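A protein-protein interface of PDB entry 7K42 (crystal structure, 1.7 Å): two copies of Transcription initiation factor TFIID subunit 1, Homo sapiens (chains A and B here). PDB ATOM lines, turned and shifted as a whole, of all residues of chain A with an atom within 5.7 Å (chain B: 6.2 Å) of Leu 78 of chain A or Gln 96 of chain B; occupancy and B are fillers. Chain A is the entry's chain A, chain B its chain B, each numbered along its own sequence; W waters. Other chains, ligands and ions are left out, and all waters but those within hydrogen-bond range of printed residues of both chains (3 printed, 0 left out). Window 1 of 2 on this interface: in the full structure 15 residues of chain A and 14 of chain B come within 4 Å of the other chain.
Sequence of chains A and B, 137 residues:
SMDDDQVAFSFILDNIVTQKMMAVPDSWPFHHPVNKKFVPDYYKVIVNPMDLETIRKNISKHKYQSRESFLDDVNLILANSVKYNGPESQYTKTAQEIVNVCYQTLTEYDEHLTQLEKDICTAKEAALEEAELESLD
The side-chain amide nitrogen (ND2) of Asn 80 of chain A sits close to the backbone carbonyl oxygen (O) of Leu 76 of chain A. The backbone carbonyl oxygen (O) of Gln 96 of chain B lies close to the side-chain amide nitrogen (ND2) of Asn 100 of chain B (3.2 Å).
Among the printed residues, pairs that only touch across the chains: Leu 78 of chain A with Leu 78 of chain B (3.6 Å), Leu 78 of chain A with Gln 96 of chain B (3.6 Å), Ala 79 of chain A with Val 82 of chain B (3.8 Å), Ala 79 of chain A with Pro 87 of chain B (3.5 Å), Ala 79 of chain A with Gln 96 of chain B (3.8 Å), Asn 80 of chain A with Pro 87 of chain B (3.6 Å), Val 82 of chain A with Val 82 of chain B (3.9 Å), Lys 83 of chain A with Val 82 of chain B (3.97 Å), Lys 83 of chain A with Pro 87 of chain B (3.7 Å), Gln 96 of chain A with Val 99 of chain B (3.9 Å) and Val 99 of chain A with Asn 100 of chain B (3.3 Å).
Printed residues of chain B that touch a printed residue of chain A: Leu 78, Val 82, Pro 87, Gln 96, Val 99 and Asn 100. Printed residues of chain A that touch a printed residue of chain B: Asn 75, Leu 78, Ala 79, Asn 80, Val 82, Lys 83, Gln 96 and Val 99.
Leu 78 of chain A touches just these residues of chain B: Leu 78 (3.6 Å) and Gln 96 (3.6 Å). Of the printed residues of chain B, Asn 80 of chain A touches Pro 87. Printed residues of chain B within 4 Å of Gln 96 of chain A: Val 99 and Asn 100. Gln 96 of chain B touches three residues of chain A. The nearest residue of chain B that does not touch Leu 78 of chain A is Val 82 of chain B (6.1 Å).
The backbone carbonyl oxygen (O) of Asn 75 of chain A lies within hydrogen-bond range of the side-chain amide nitrogen (NE2) of Gln 96 of chain B. OD1 of Asn 75 of chain A lies within hydrogen-bond range of ND2 of Asn 100 of chain B (3.0 Å). NE2 of Gln 96 of chain A sits at hydrogen-bond distance from OD1 of Asn 100 of chain B.
Water W3 bridges the backbone carbonyl oxygen (O) of Lys 93 of chain B (2.7 Å) and the side-chain amide nitrogen (ND2) of Asn 75 of chain A (3.3 Å). Water W1 lies within hydrogen-bond range of the side-chain carboxylate of Glu 97 of chain B (2.7 Å), the side-chain amide nitrogen of Asn 100 of chain B (3.0 Å) and the side-chain amide nitrogen of Asn 75 of chain A (3.0 Å). Water W2 lies within hydrogen-bond range of the side-chain amide oxygen (OD1) of Asn 100 of chain B (2.9 Å), the side-chain amide oxygen (OE1) of Gln 96 of chain A (3.0 Å) and the side-chain amide nitrogen (NE2) of Gln 96 of chain B (3.4 Å).
Leu 78 of chain A touches its own counterpart, Leu 78 of chain B. Leu 78 of chain A touches Gln 96 of chain B, but with the chains exchanged Gln 96 of chain A does not touch Leu 78 of chain B (4.6 Å). Val 82 of chain B touches its own counterpart, Val 82 of chain A. Gln 96 of chain A touches Val 99 of chain B, but with the chains exchanged Val 99 of chain A does not touch Gln 96 of chain B (5.3 Å). Positions printed for both chains: 78, 82, 92, 93, 95, 96 and 99. Of the 14 pairs that touch across the chains among the printed residues, 2 have their exchanged pair printed and touching as well.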
ATOM      1  N   VAL A  74       1.744   2.198   1.463  1.00  0.00           N
ATOM      2  CA  VAL A  74       1.153   2.594   0.187  1.00  0.00           C
ATOM      3  C   VAL A  74       2.223   2.628  -0.894  1.00  0.00           C
ATOM      4  O   VAL A  74       2.042   2.107  -2.000  1.00  0.00           O
ATOM      5  CB  VAL A  74       0.457   3.961   0.321  1.00  0.00           C
ATOM      6  CG1 VAL A  74       0.048   4.490  -1.065  1.00  0.00           C
ATOM      7  CG2 VAL A  74      -0.775   3.845   1.260  1.00  0.00           C
ATOM      8  N   ASN A  75       3.362   3.252  -0.586  1.00  0.00           N
ATOM      9  CA  ASN A  75       4.430   3.333  -1.577  1.00  0.00           C
ATOM     10  C   ASN A  75       4.944   1.954  -1.960  1.00  0.00           C
ATOM     11  O   ASN A  75       5.378   1.748  -3.097  1.00  0.00           O
ATOM     12  CB  ASN A  75       5.587   4.171  -1.033  1.00  0.00           C
ATOM     13  CG  ASN A  75       5.367   5.646  -1.206  1.00  0.00           C
ATOM     14  OD1 ASN A  75       4.788   6.079  -2.201  1.00  0.00           O
ATOM     15  ND2 ASN A  75       5.867   6.441  -0.255  1.00  0.00           N
ATOM     16  N   LEU A  76       4.900   0.997  -1.032  1.00  0.00           N
ATOM     17  CA  LEU A  76       5.388  -0.346  -1.343  1.00  0.00           C
ATOM     18  C   LEU A  76       4.558  -1.000  -2.443  1.00  0.00           C
ATOM     19  O   LEU A  76       5.084  -1.791  -3.236  1.00  0.00           O
ATOM     20  CB  LEU A  76       5.379  -1.204  -0.079  1.00  0.00           C
ATOM     21  CG  LEU A  76       5.847  -2.657  -0.216  1.00  0.00           C
ATOM     22  CD1 LEU A  76       7.262  -2.748  -0.792  1.00  0.00           C
ATOM     23  CD2 LEU A  76       5.778  -3.317   1.172  1.00  0.00           C
ATOM     24  N   ILE A  77       3.262  -0.701  -2.493  1.00  0.00           N
ATOM     25  CA  ILE A  77       2.427  -1.203  -3.584  1.00  0.00           C
ATOM     26  C   ILE A  77       3.010  -0.786  -4.929  1.00  0.00           C
ATOM     27  O   ILE A  77       3.116  -1.594  -5.860  1.00  0.00           O
ATOM     28  CB  ILE A  77       0.981  -0.705  -3.417  1.00  0.00           C
ATOM     29  CG1 ILE A  77       0.385  -1.268  -2.121  1.00  0.00           C
ATOM     30  CG2 ILE A  77       0.136  -1.091  -4.638  1.00  0.00           C
ATOM     31  CD1 ILE A  77      -1.026  -0.769  -1.825  1.00  0.00           C
ATOM     32  N   LEU A  78       3.398   0.488  -5.051  1.00  0.00           N
ATOM     33  CA  LEU A  78       3.949   0.969  -6.317  1.00  0.00           C
ATOM     34  C   LEU A  78       5.318   0.353  -6.597  1.00  0.00           C
ATOM     35  O   LEU A  78       5.589  -0.120  -7.711  1.00  0.00           O
ATOM     36  CB  LEU A  78       4.029   2.503  -6.294  1.00  0.00           C
ATOM     37  CG  LEU A  78       4.590   3.285  -7.501  1.00  0.00           C
ATOM     38  CD1 LEU A  78       6.121   3.325  -7.530  1.00  0.00           C
ATOM     39  CD2 LEU A  78       4.042   2.744  -8.818  1.00  0.00           C
ATOM     40  N   ALA A  79       6.197   0.348  -5.598  1.00  0.00           N
ATOM     41  CA  ALA A  79       7.537  -0.200  -5.799  1.00  0.00           C
ATOM     42  C   ALA A  79       7.471  -1.666  -6.203  1.00  0.00           C
ATOM     43  O   ALA A  79       8.227  -2.112  -7.074  1.00  0.00           O
ATOM     44  CB  ALA A  79       8.386  -0.004  -4.536  1.00  0.00           C
ATOM     45  N   ASN A  80       6.567  -2.434  -5.587  1.00  0.00           N
ATOM     46  CA  ASN A  80       6.412  -3.829  -5.984  1.00  0.00           C
ATOM     47  C   ASN A  80       5.922  -3.932  -7.415  1.00  0.00           C
ATOM     48  O   ASN A  80       6.330  -4.837  -8.149  1.00  0.00           O
ATOM     49  CB  ASN A  80       5.441  -4.558  -5.057  1.00  0.00           C
ATOM     50  CG  ASN A  80       6.069  -4.924  -3.724  1.00  0.00           C
ATOM     51  OD1 ASN A  80       7.292  -4.988  -3.596  1.00  0.00           O
ATOM     52  ND2 ASN A  80       5.228  -5.174  -2.723  1.00  0.00           N
ATOM     53  N   SER A  81       5.055  -3.007  -7.839  1.00  0.00           N
ATOM     54  CA  SER A  81       4.561  -3.098  -9.208  1.00  0.00           C
ATOM     55  C   SER A  81       5.660  -2.724 -10.199  1.00  0.00           C
ATOM     56  O   SER A  81       5.743  -3.316 -11.278  1.00  0.00           O
ATOM     57  CB  SER A  81       3.344  -2.191  -9.400  1.00  0.00           C
ATOM     58  OG  SER A  81       2.918  -2.145 -10.761  1.00  0.00           O
ATOM     59  N   VAL A  82       6.549  -1.792  -9.830  1.00  0.00           N
ATOM     60  CA  VAL A  82       7.709  -1.509 -10.677  1.00  0.00           C
ATOM     61  C   VAL A  82       8.529  -2.773 -10.873  1.00  0.00           C
ATOM     62  O   VAL A  82       8.948  -3.095 -11.992  1.00  0.00           O
ATOM     63  CB  VAL A  82       8.561  -0.374 -10.068  1.00  0.00           C
ATOM     64  CG1 VAL A  82       9.894  -0.231 -10.830  1.00  0.00           C
ATOM     65  CG2 VAL A  82       7.789   0.925 -10.095  1.00  0.00           C
ATOM     66  N   LYS A  83       8.755  -3.521  -9.788  1.00  0.00           N
ATOM     67  CA  LYS A  83       9.566  -4.733  -9.867  1.00  0.00           C
ATOM     68  C   LYS A  83       8.864  -5.835 -10.657  1.00  0.00           C
ATOM     69  O   LYS A  83       9.486  -6.489 -11.509  1.00  0.00           O
ATOM     70  CB  LYS A  83       9.920  -5.222  -8.461  1.00  0.00           C
ATOM     71  CG  LYS A  83      10.751  -6.507  -8.463  1.00  0.00           C
ATOM     72  CD  LYS A  83      11.231  -6.877  -7.073  1.00  0.00           C
ATOM     73  CE  LYS A  83      12.028  -8.172  -7.103  1.00  0.00           C
ATOM     74  NZ  LYS A  83      12.399  -8.622  -5.730  1.00  0.00           N
ATOM     75  N   THR A  92       1.624  -0.255 -13.326  1.00  0.00           N
ATOM     76  CA  THR A  92       2.440   0.656 -12.533  1.00  0.00           C
ATOM     77  C   THR A  92       1.912   2.083 -12.608  1.00  0.00           C
ATOM     78  O   THR A  92       1.920   2.805 -11.605  1.00  0.00           O
ATOM     79  CB  THR A  92       3.880   0.543 -13.015  1.00  0.00           C
ATOM     80  OG1 THR A  92       4.318  -0.797 -12.751  1.00  0.00           O
ATOM     81  CG2 THR A  92       4.801   1.549 -12.306  1.00  0.00           C
ATOM     82  N   LYS A  93       1.421   2.501 -13.779  1.00  0.00           N
ATOM     83  CA  LYS A  93       0.827   3.831 -13.874  1.00  0.00           C
ATOM     84  C   LYS A  93      -0.408   3.932 -12.990  1.00  0.00           C
ATOM     85  O   LYS A  93      -0.621   4.948 -12.321  1.00  0.00           O
ATOM     86  CB  LYS A  93       0.491   4.166 -15.329  1.00  0.00           C
ATOM     87  CG  LYS A  93       1.729   4.266 -16.213  1.00  0.00           C
ATOM     88  CD  LYS A  93       1.397   4.708 -17.644  1.00  0.00           C
ATOM     89  CE  LYS A  93       2.658   4.727 -18.513  1.00  0.00           C
ATOM     90  NZ  LYS A  93       3.638   5.757 -18.045  1.00  0.00           N
ATOM     91  N   ALA A  95      -0.913   2.105 -10.250  1.00  0.00           N
ATOM     92  CA  ALA A  95      -0.410   2.157  -8.879  1.00  0.00           C
ATOM     93  C   ALA A  95       0.106   3.547  -8.526  1.00  0.00           C
ATOM     94  O   ALA A  95      -0.096   4.016  -7.400  1.00  0.00           O
ATOM     95  CB  ALA A  95       0.694   1.119  -8.670  1.00  0.00           C
ATOM     96  N   GLN A  96       0.775   4.227  -9.466  1.00  0.00           N
ATOM     97  CA  GLN A  96       1.259   5.571  -9.146  1.00  0.00           C
ATOM     98  C   GLN A  96       0.106   6.545  -8.936  1.00  0.00           C
ATOM     99  O   GLN A  96       0.219   7.471  -8.125  1.00  0.00           O
ATOM    100  CB  GLN A  96       2.198   6.092 -10.241  1.00  0.00           C
ATOM    101  CG  GLN A  96       2.816   7.479  -9.918  1.00  0.00           C
ATOM    102  CD  GLN A  96       3.725   7.466  -8.687  1.00  0.00           C
ATOM    103  OE1 GLN A  96       4.662   6.683  -8.617  1.00  0.00           O
ATOM    104  NE2 GLN A  96       3.463   8.358  -7.727  1.00  0.00           N
ATOM    105  N   VAL A  99      -0.969   6.006  -5.468  1.00  0.00           N
ATOM    106  CA  VAL A  99      -0.045   6.708  -4.573  1.00  0.00           C
ATOM    107  C   VAL A  99      -0.322   8.203  -4.606  1.00  0.00           C
ATOM    108  O   VAL A  99      -0.371   8.866  -3.560  1.00  0.00           O
ATOM    109  CB  VAL A  99       1.420   6.408  -4.959  1.00  0.00           C
ATOM    110  CG1 VAL A  99       2.380   7.330  -4.200  1.00  0.00           C
ATOM    111  CG2 VAL A  99       1.768   4.967  -4.671  1.00  0.00           C
ATOM    112  N   LEU B  78      13.470   6.386 -10.125  1.00  0.00           N
ATOM    113  CA  LEU B  78      12.828   5.434  -9.223  1.00  0.00           C
ATOM    114  C   LEU B  78      12.990   4.007  -9.731  1.00  0.00           C
ATOM    115  O   LEU B  78      13.281   3.090  -8.950  1.00  0.00           O
ATOM    116  CB  LEU B  78      11.349   5.791  -9.068  1.00  0.00           C
ATOM    117  CG  LEU B  78      10.487   4.817  -8.266  1.00  0.00           C
ATOM    118  CD1 LEU B  78      11.116   4.506  -6.902  1.00  0.00           C
ATOM    119  CD2 LEU B  78       9.066   5.371  -8.108  1.00  0.00           C
ATOM    120  N   VAL B  82      14.568   0.902  -7.612  1.00  0.00           N
ATOM    121  CA  VAL B  82      13.907  -0.370  -7.330  1.00  0.00           C
ATOM    122  C   VAL B  82      14.801  -1.528  -7.753  1.00  0.00           C
ATOM    123  O   VAL B  82      14.942  -2.523  -7.030  1.00  0.00           O
ATOM    124  CB  VAL B  82      12.531  -0.435  -8.020  1.00  0.00           C
ATOM    125  CG1 VAL B  82      11.929  -1.855  -7.865  1.00  0.00           C
ATOM    126  CG2 VAL B  82      11.593   0.598  -7.416  1.00  0.00           C
ATOM    127  N   PRO B  87      12.700  -2.835  -3.683  1.00  0.00           N
ATOM    128  CA  PRO B  87      11.462  -2.059  -3.472  1.00  0.00           C
ATOM    129  C   PRO B  87      11.301  -1.486  -2.070  1.00  0.00           C
ATOM    130  O   PRO B  87      10.616  -0.468  -1.925  1.00  0.00           O
ATOM    131  CB  PRO B  87      10.344  -3.074  -3.765  1.00  0.00           C
ATOM    132  CG  PRO B  87      10.979  -4.195  -4.475  1.00  0.00           C
ATOM    133  CD  PRO B  87      12.449  -4.198  -4.199  1.00  0.00           C
ATOM    134  N   TYR B  91      16.662   3.879   0.263  1.00  0.00           N
ATOM    135  CA  TYR B  91      16.953   4.711  -0.899  1.00  0.00           C
ATOM    136  C   TYR B  91      15.757   4.770  -1.832  1.00  0.00           C
ATOM    137  O   TYR B  91      15.464   5.823  -2.405  1.00  0.00           O
ATOM    138  CB  TYR B  91      18.191   4.179  -1.631  1.00  0.00           C
ATOM    139  CG  TYR B  91      19.431   4.297  -0.769  1.00  0.00           C
ATOM    140  CD1 TYR B  91      20.085   5.513  -0.629  1.00  0.00           C
ATOM    141  CD2 TYR B  91      19.929   3.193  -0.070  1.00  0.00           C
ATOM    142  CE1 TYR B  91      21.208   5.629   0.176  1.00  0.00           C
ATOM    143  CE2 TYR B  91      21.044   3.301   0.737  1.00  0.00           C
ATOM    144  CZ  TYR B  91      21.682   4.520   0.854  1.00  0.00           C
ATOM    145  OH  TYR B  91      22.796   4.631   1.661  1.00  0.00           O
ATOM    146  N   THR B  92      15.050   3.651  -1.987  1.00  0.00           N
ATOM    147  CA  THR B  92      13.862   3.660  -2.829  1.00  0.00           C
ATOM    148  C   THR B  92      12.761   4.502  -2.202  1.00  0.00           C
ATOM    149  O   THR B  92      12.027   5.204  -2.911  1.00  0.00           O
ATOM    150  CB  THR B  92      13.403   2.227  -3.072  1.00  0.00           C
ATOM    151  OG1 THR B  92      14.429   1.547  -3.794  1.00  0.00           O
ATOM    152  CG2 THR B  92      12.072   2.185  -3.873  1.00  0.00           C
ATOM    153  N   LYS B  93      12.645   4.471  -0.872  1.00  0.00           N
ATOM    154  CA  LYS B  93      11.658   5.328  -0.225  1.00  0.00           C
ATOM    155  C   LYS B  93      11.976   6.794  -0.468  1.00  0.00           C
ATOM    156  O   LYS B  93      11.073   7.593  -0.734  1.00  0.00           O
ATOM    157  CB  LYS B  93      11.591   5.036   1.277  1.00  0.00           C
ATOM    158  CG  LYS B  93      11.081   3.630   1.584  1.00  0.00           C
ATOM    159  CD  LYS B  93      10.804   3.441   3.064  1.00  0.00           C
ATOM    160  CE  LYS B  93      12.062   3.102   3.837  1.00  0.00           C
ATOM    161  NZ  LYS B  93      11.713   2.366   5.089  1.00  0.00           N
ATOM    162  N   THR B  94      13.262   7.169  -0.391  1.00  0.00           N
ATOM    163  CA  THR B  94      13.652   8.540  -0.718  1.00  0.00           C
ATOM    164  C   THR B  94      13.312   8.873  -2.168  1.00  0.00           C
ATOM    165  O   THR B  94      12.762   9.944  -2.462  1.00  0.00           O
ATOM    166  CB  THR B  94      15.145   8.729  -0.441  1.00  0.00           C
ATOM    167  OG1 THR B  94      15.382   8.521   0.964  1.00  0.00           O
ATOM    168  CG2 THR B  94      15.599  10.158  -0.815  1.00  0.00           C
ATOM    169  N   ALA B  95      13.627   7.962  -3.093  1.00  0.00           N
ATOM    170  CA  ALA B  95      13.282   8.200  -4.493  1.00  0.00           C
ATOM    171  C   ALA B  95      11.775   8.364  -4.674  1.00  0.00           C
ATOM    172  O   ALA B  95      11.324   9.163  -5.504  1.00  0.00           O
ATOM    173  CB  ALA B  95      13.793   7.051  -5.374  1.00  0.00           C
ATOM    174  N   GLN B  96      10.980   7.607  -3.919  1.00  0.00           N
ATOM    175  CA  GLN B  96       9.531   7.724  -4.067  1.00  0.00           C
ATOM    176  C   GLN B  96       9.024   9.048  -3.533  1.00  0.00           C
ATOM    177  O   GLN B  96       8.067   9.605  -4.080  1.00  0.00           O
ATOM    178  CB  GLN B  96       8.832   6.551  -3.378  1.00  0.00           C
ATOM    179  CG  GLN B  96       8.976   5.281  -4.199  1.00  0.00           C
ATOM    180  CD  GLN B  96       8.200   4.111  -3.632  1.00  0.00           C
ATOM    181  OE1 GLN B  96       8.696   3.397  -2.774  1.00  0.00           O
ATOM    182  NE2 GLN B  96       6.977   3.913  -4.119  1.00  0.00           N
ATOM    183  N   GLU B  97       9.646   9.580  -2.476  1.00  0.00           N
ATOM    184  CA  GLU B  97       9.247  10.914  -2.030  1.00  0.00           C
ATOM    185  C   GLU B  97       9.580  11.960  -3.092  1.00  0.00           C
ATOM    186  O   GLU B  97       8.793  12.884  -3.331  1.00  0.00           O
ATOM    187  CB  GLU B  97       9.926  11.240  -0.698  1.00  0.00           C
ATOM    188  CG  GLU B  97       9.599  12.625  -0.135  1.00  0.00           C
ATOM    189  CD  GLU B  97       8.161  12.775   0.343  1.00  0.00           C
ATOM    190  OE1 GLU B  97       7.510  11.751   0.694  1.00  0.00           O
ATOM    191  OE2 GLU B  97       7.687  13.937   0.366  1.00  0.00           O
ATOM    192  N   ILE B  98      10.726  11.805  -3.759  1.00  0.00           N
ATOM    193  CA  ILE B  98      11.098  12.673  -4.878  1.00  0.00           C
ATOM    194  C   ILE B  98      10.058  12.595  -5.996  1.00  0.00           C
ATOM    195  O   ILE B  98       9.604  13.622  -6.516  1.00  0.00           O
ATOM    196  CB  ILE B  98      12.498  12.287  -5.394  1.00  0.00           C
ATOM    197  CG1 ILE B  98      13.564  12.631  -4.349  1.00  0.00           C
ATOM    198  CG2 ILE B  98      12.791  12.995  -6.737  1.00  0.00           C
ATOM    199  CD1 ILE B  98      14.976  12.055  -4.677  1.00  0.00           C
ATOM    200  N   VAL B  99       9.692  11.373  -6.406  1.00  0.00           N
ATOM    201  CA  VAL B  99       8.688  11.208  -7.453  1.00  0.00           C
ATOM    202  C   VAL B  99       7.345  11.756  -6.989  1.00  0.00           C
ATOM    203  O   VAL B  99       6.636  12.444  -7.744  1.00  0.00           O
ATOM    204  CB  VAL B  99       8.579   9.723  -7.860  1.00  0.00           C
ATOM    205  CG1 VAL B  99       7.364   9.472  -8.778  1.00  0.00           C
ATOM    206  CG2 VAL B  99       9.865   9.277  -8.546  1.00  0.00           C
ATOM    207  N   ASN B 100       6.955  11.439  -5.749  1.00  0.00           N
ATOM    208  CA  ASN B 100       5.618  11.816  -5.290  1.00  0.00           C
ATOM    209  C   ASN B 100       5.467  13.327  -5.194  1.00  0.00           C
ATOM    210  O   ASN B 100       4.420  13.872  -5.561  1.00  0.00           O
ATOM    211  CB  ASN B 100       5.307  11.165  -3.941  1.00  0.00           C
ATOM    212  CG  ASN B 100       5.134   9.658  -4.049  1.00  0.00           C
ATOM    213  OD1 ASN B 100       4.991   9.113  -5.143  1.00  0.00           O
ATOM    214  ND2 ASN B 100       5.164   8.975  -2.905  1.00  0.00           N
ATOM    215  N   VAL B 101       6.489  14.018  -4.679  1.00  0.00           N
ATOM    216  CA  VAL B 101       6.366  15.469  -4.581  1.00  0.00           C
ATOM    217  C   VAL B 101       6.421  16.090  -5.966  1.00  0.00           C
ATOM    218  O   VAL B 101       5.821  17.144  -6.201  1.00  0.00           O
ATOM    219  CB  VAL B 101       7.433  16.063  -3.635  1.00  0.00           C
ATOM    220  CG1 VAL B 101       8.810  16.144  -4.310  1.00  0.00           C
ATOM    221  CG2 VAL B 101       7.006  17.453  -3.192  1.00  0.00           C
HETATM  222  O   HOH W   1       6.625   9.361  -0.337  1.00  0.00           O
HETATM  223  O   HOH W   2       6.230   6.675  -6.020  1.00  0.00           O
HETATM  224  O   HOH W   3       8.782   7.713   0.601  1.00  0.00           O
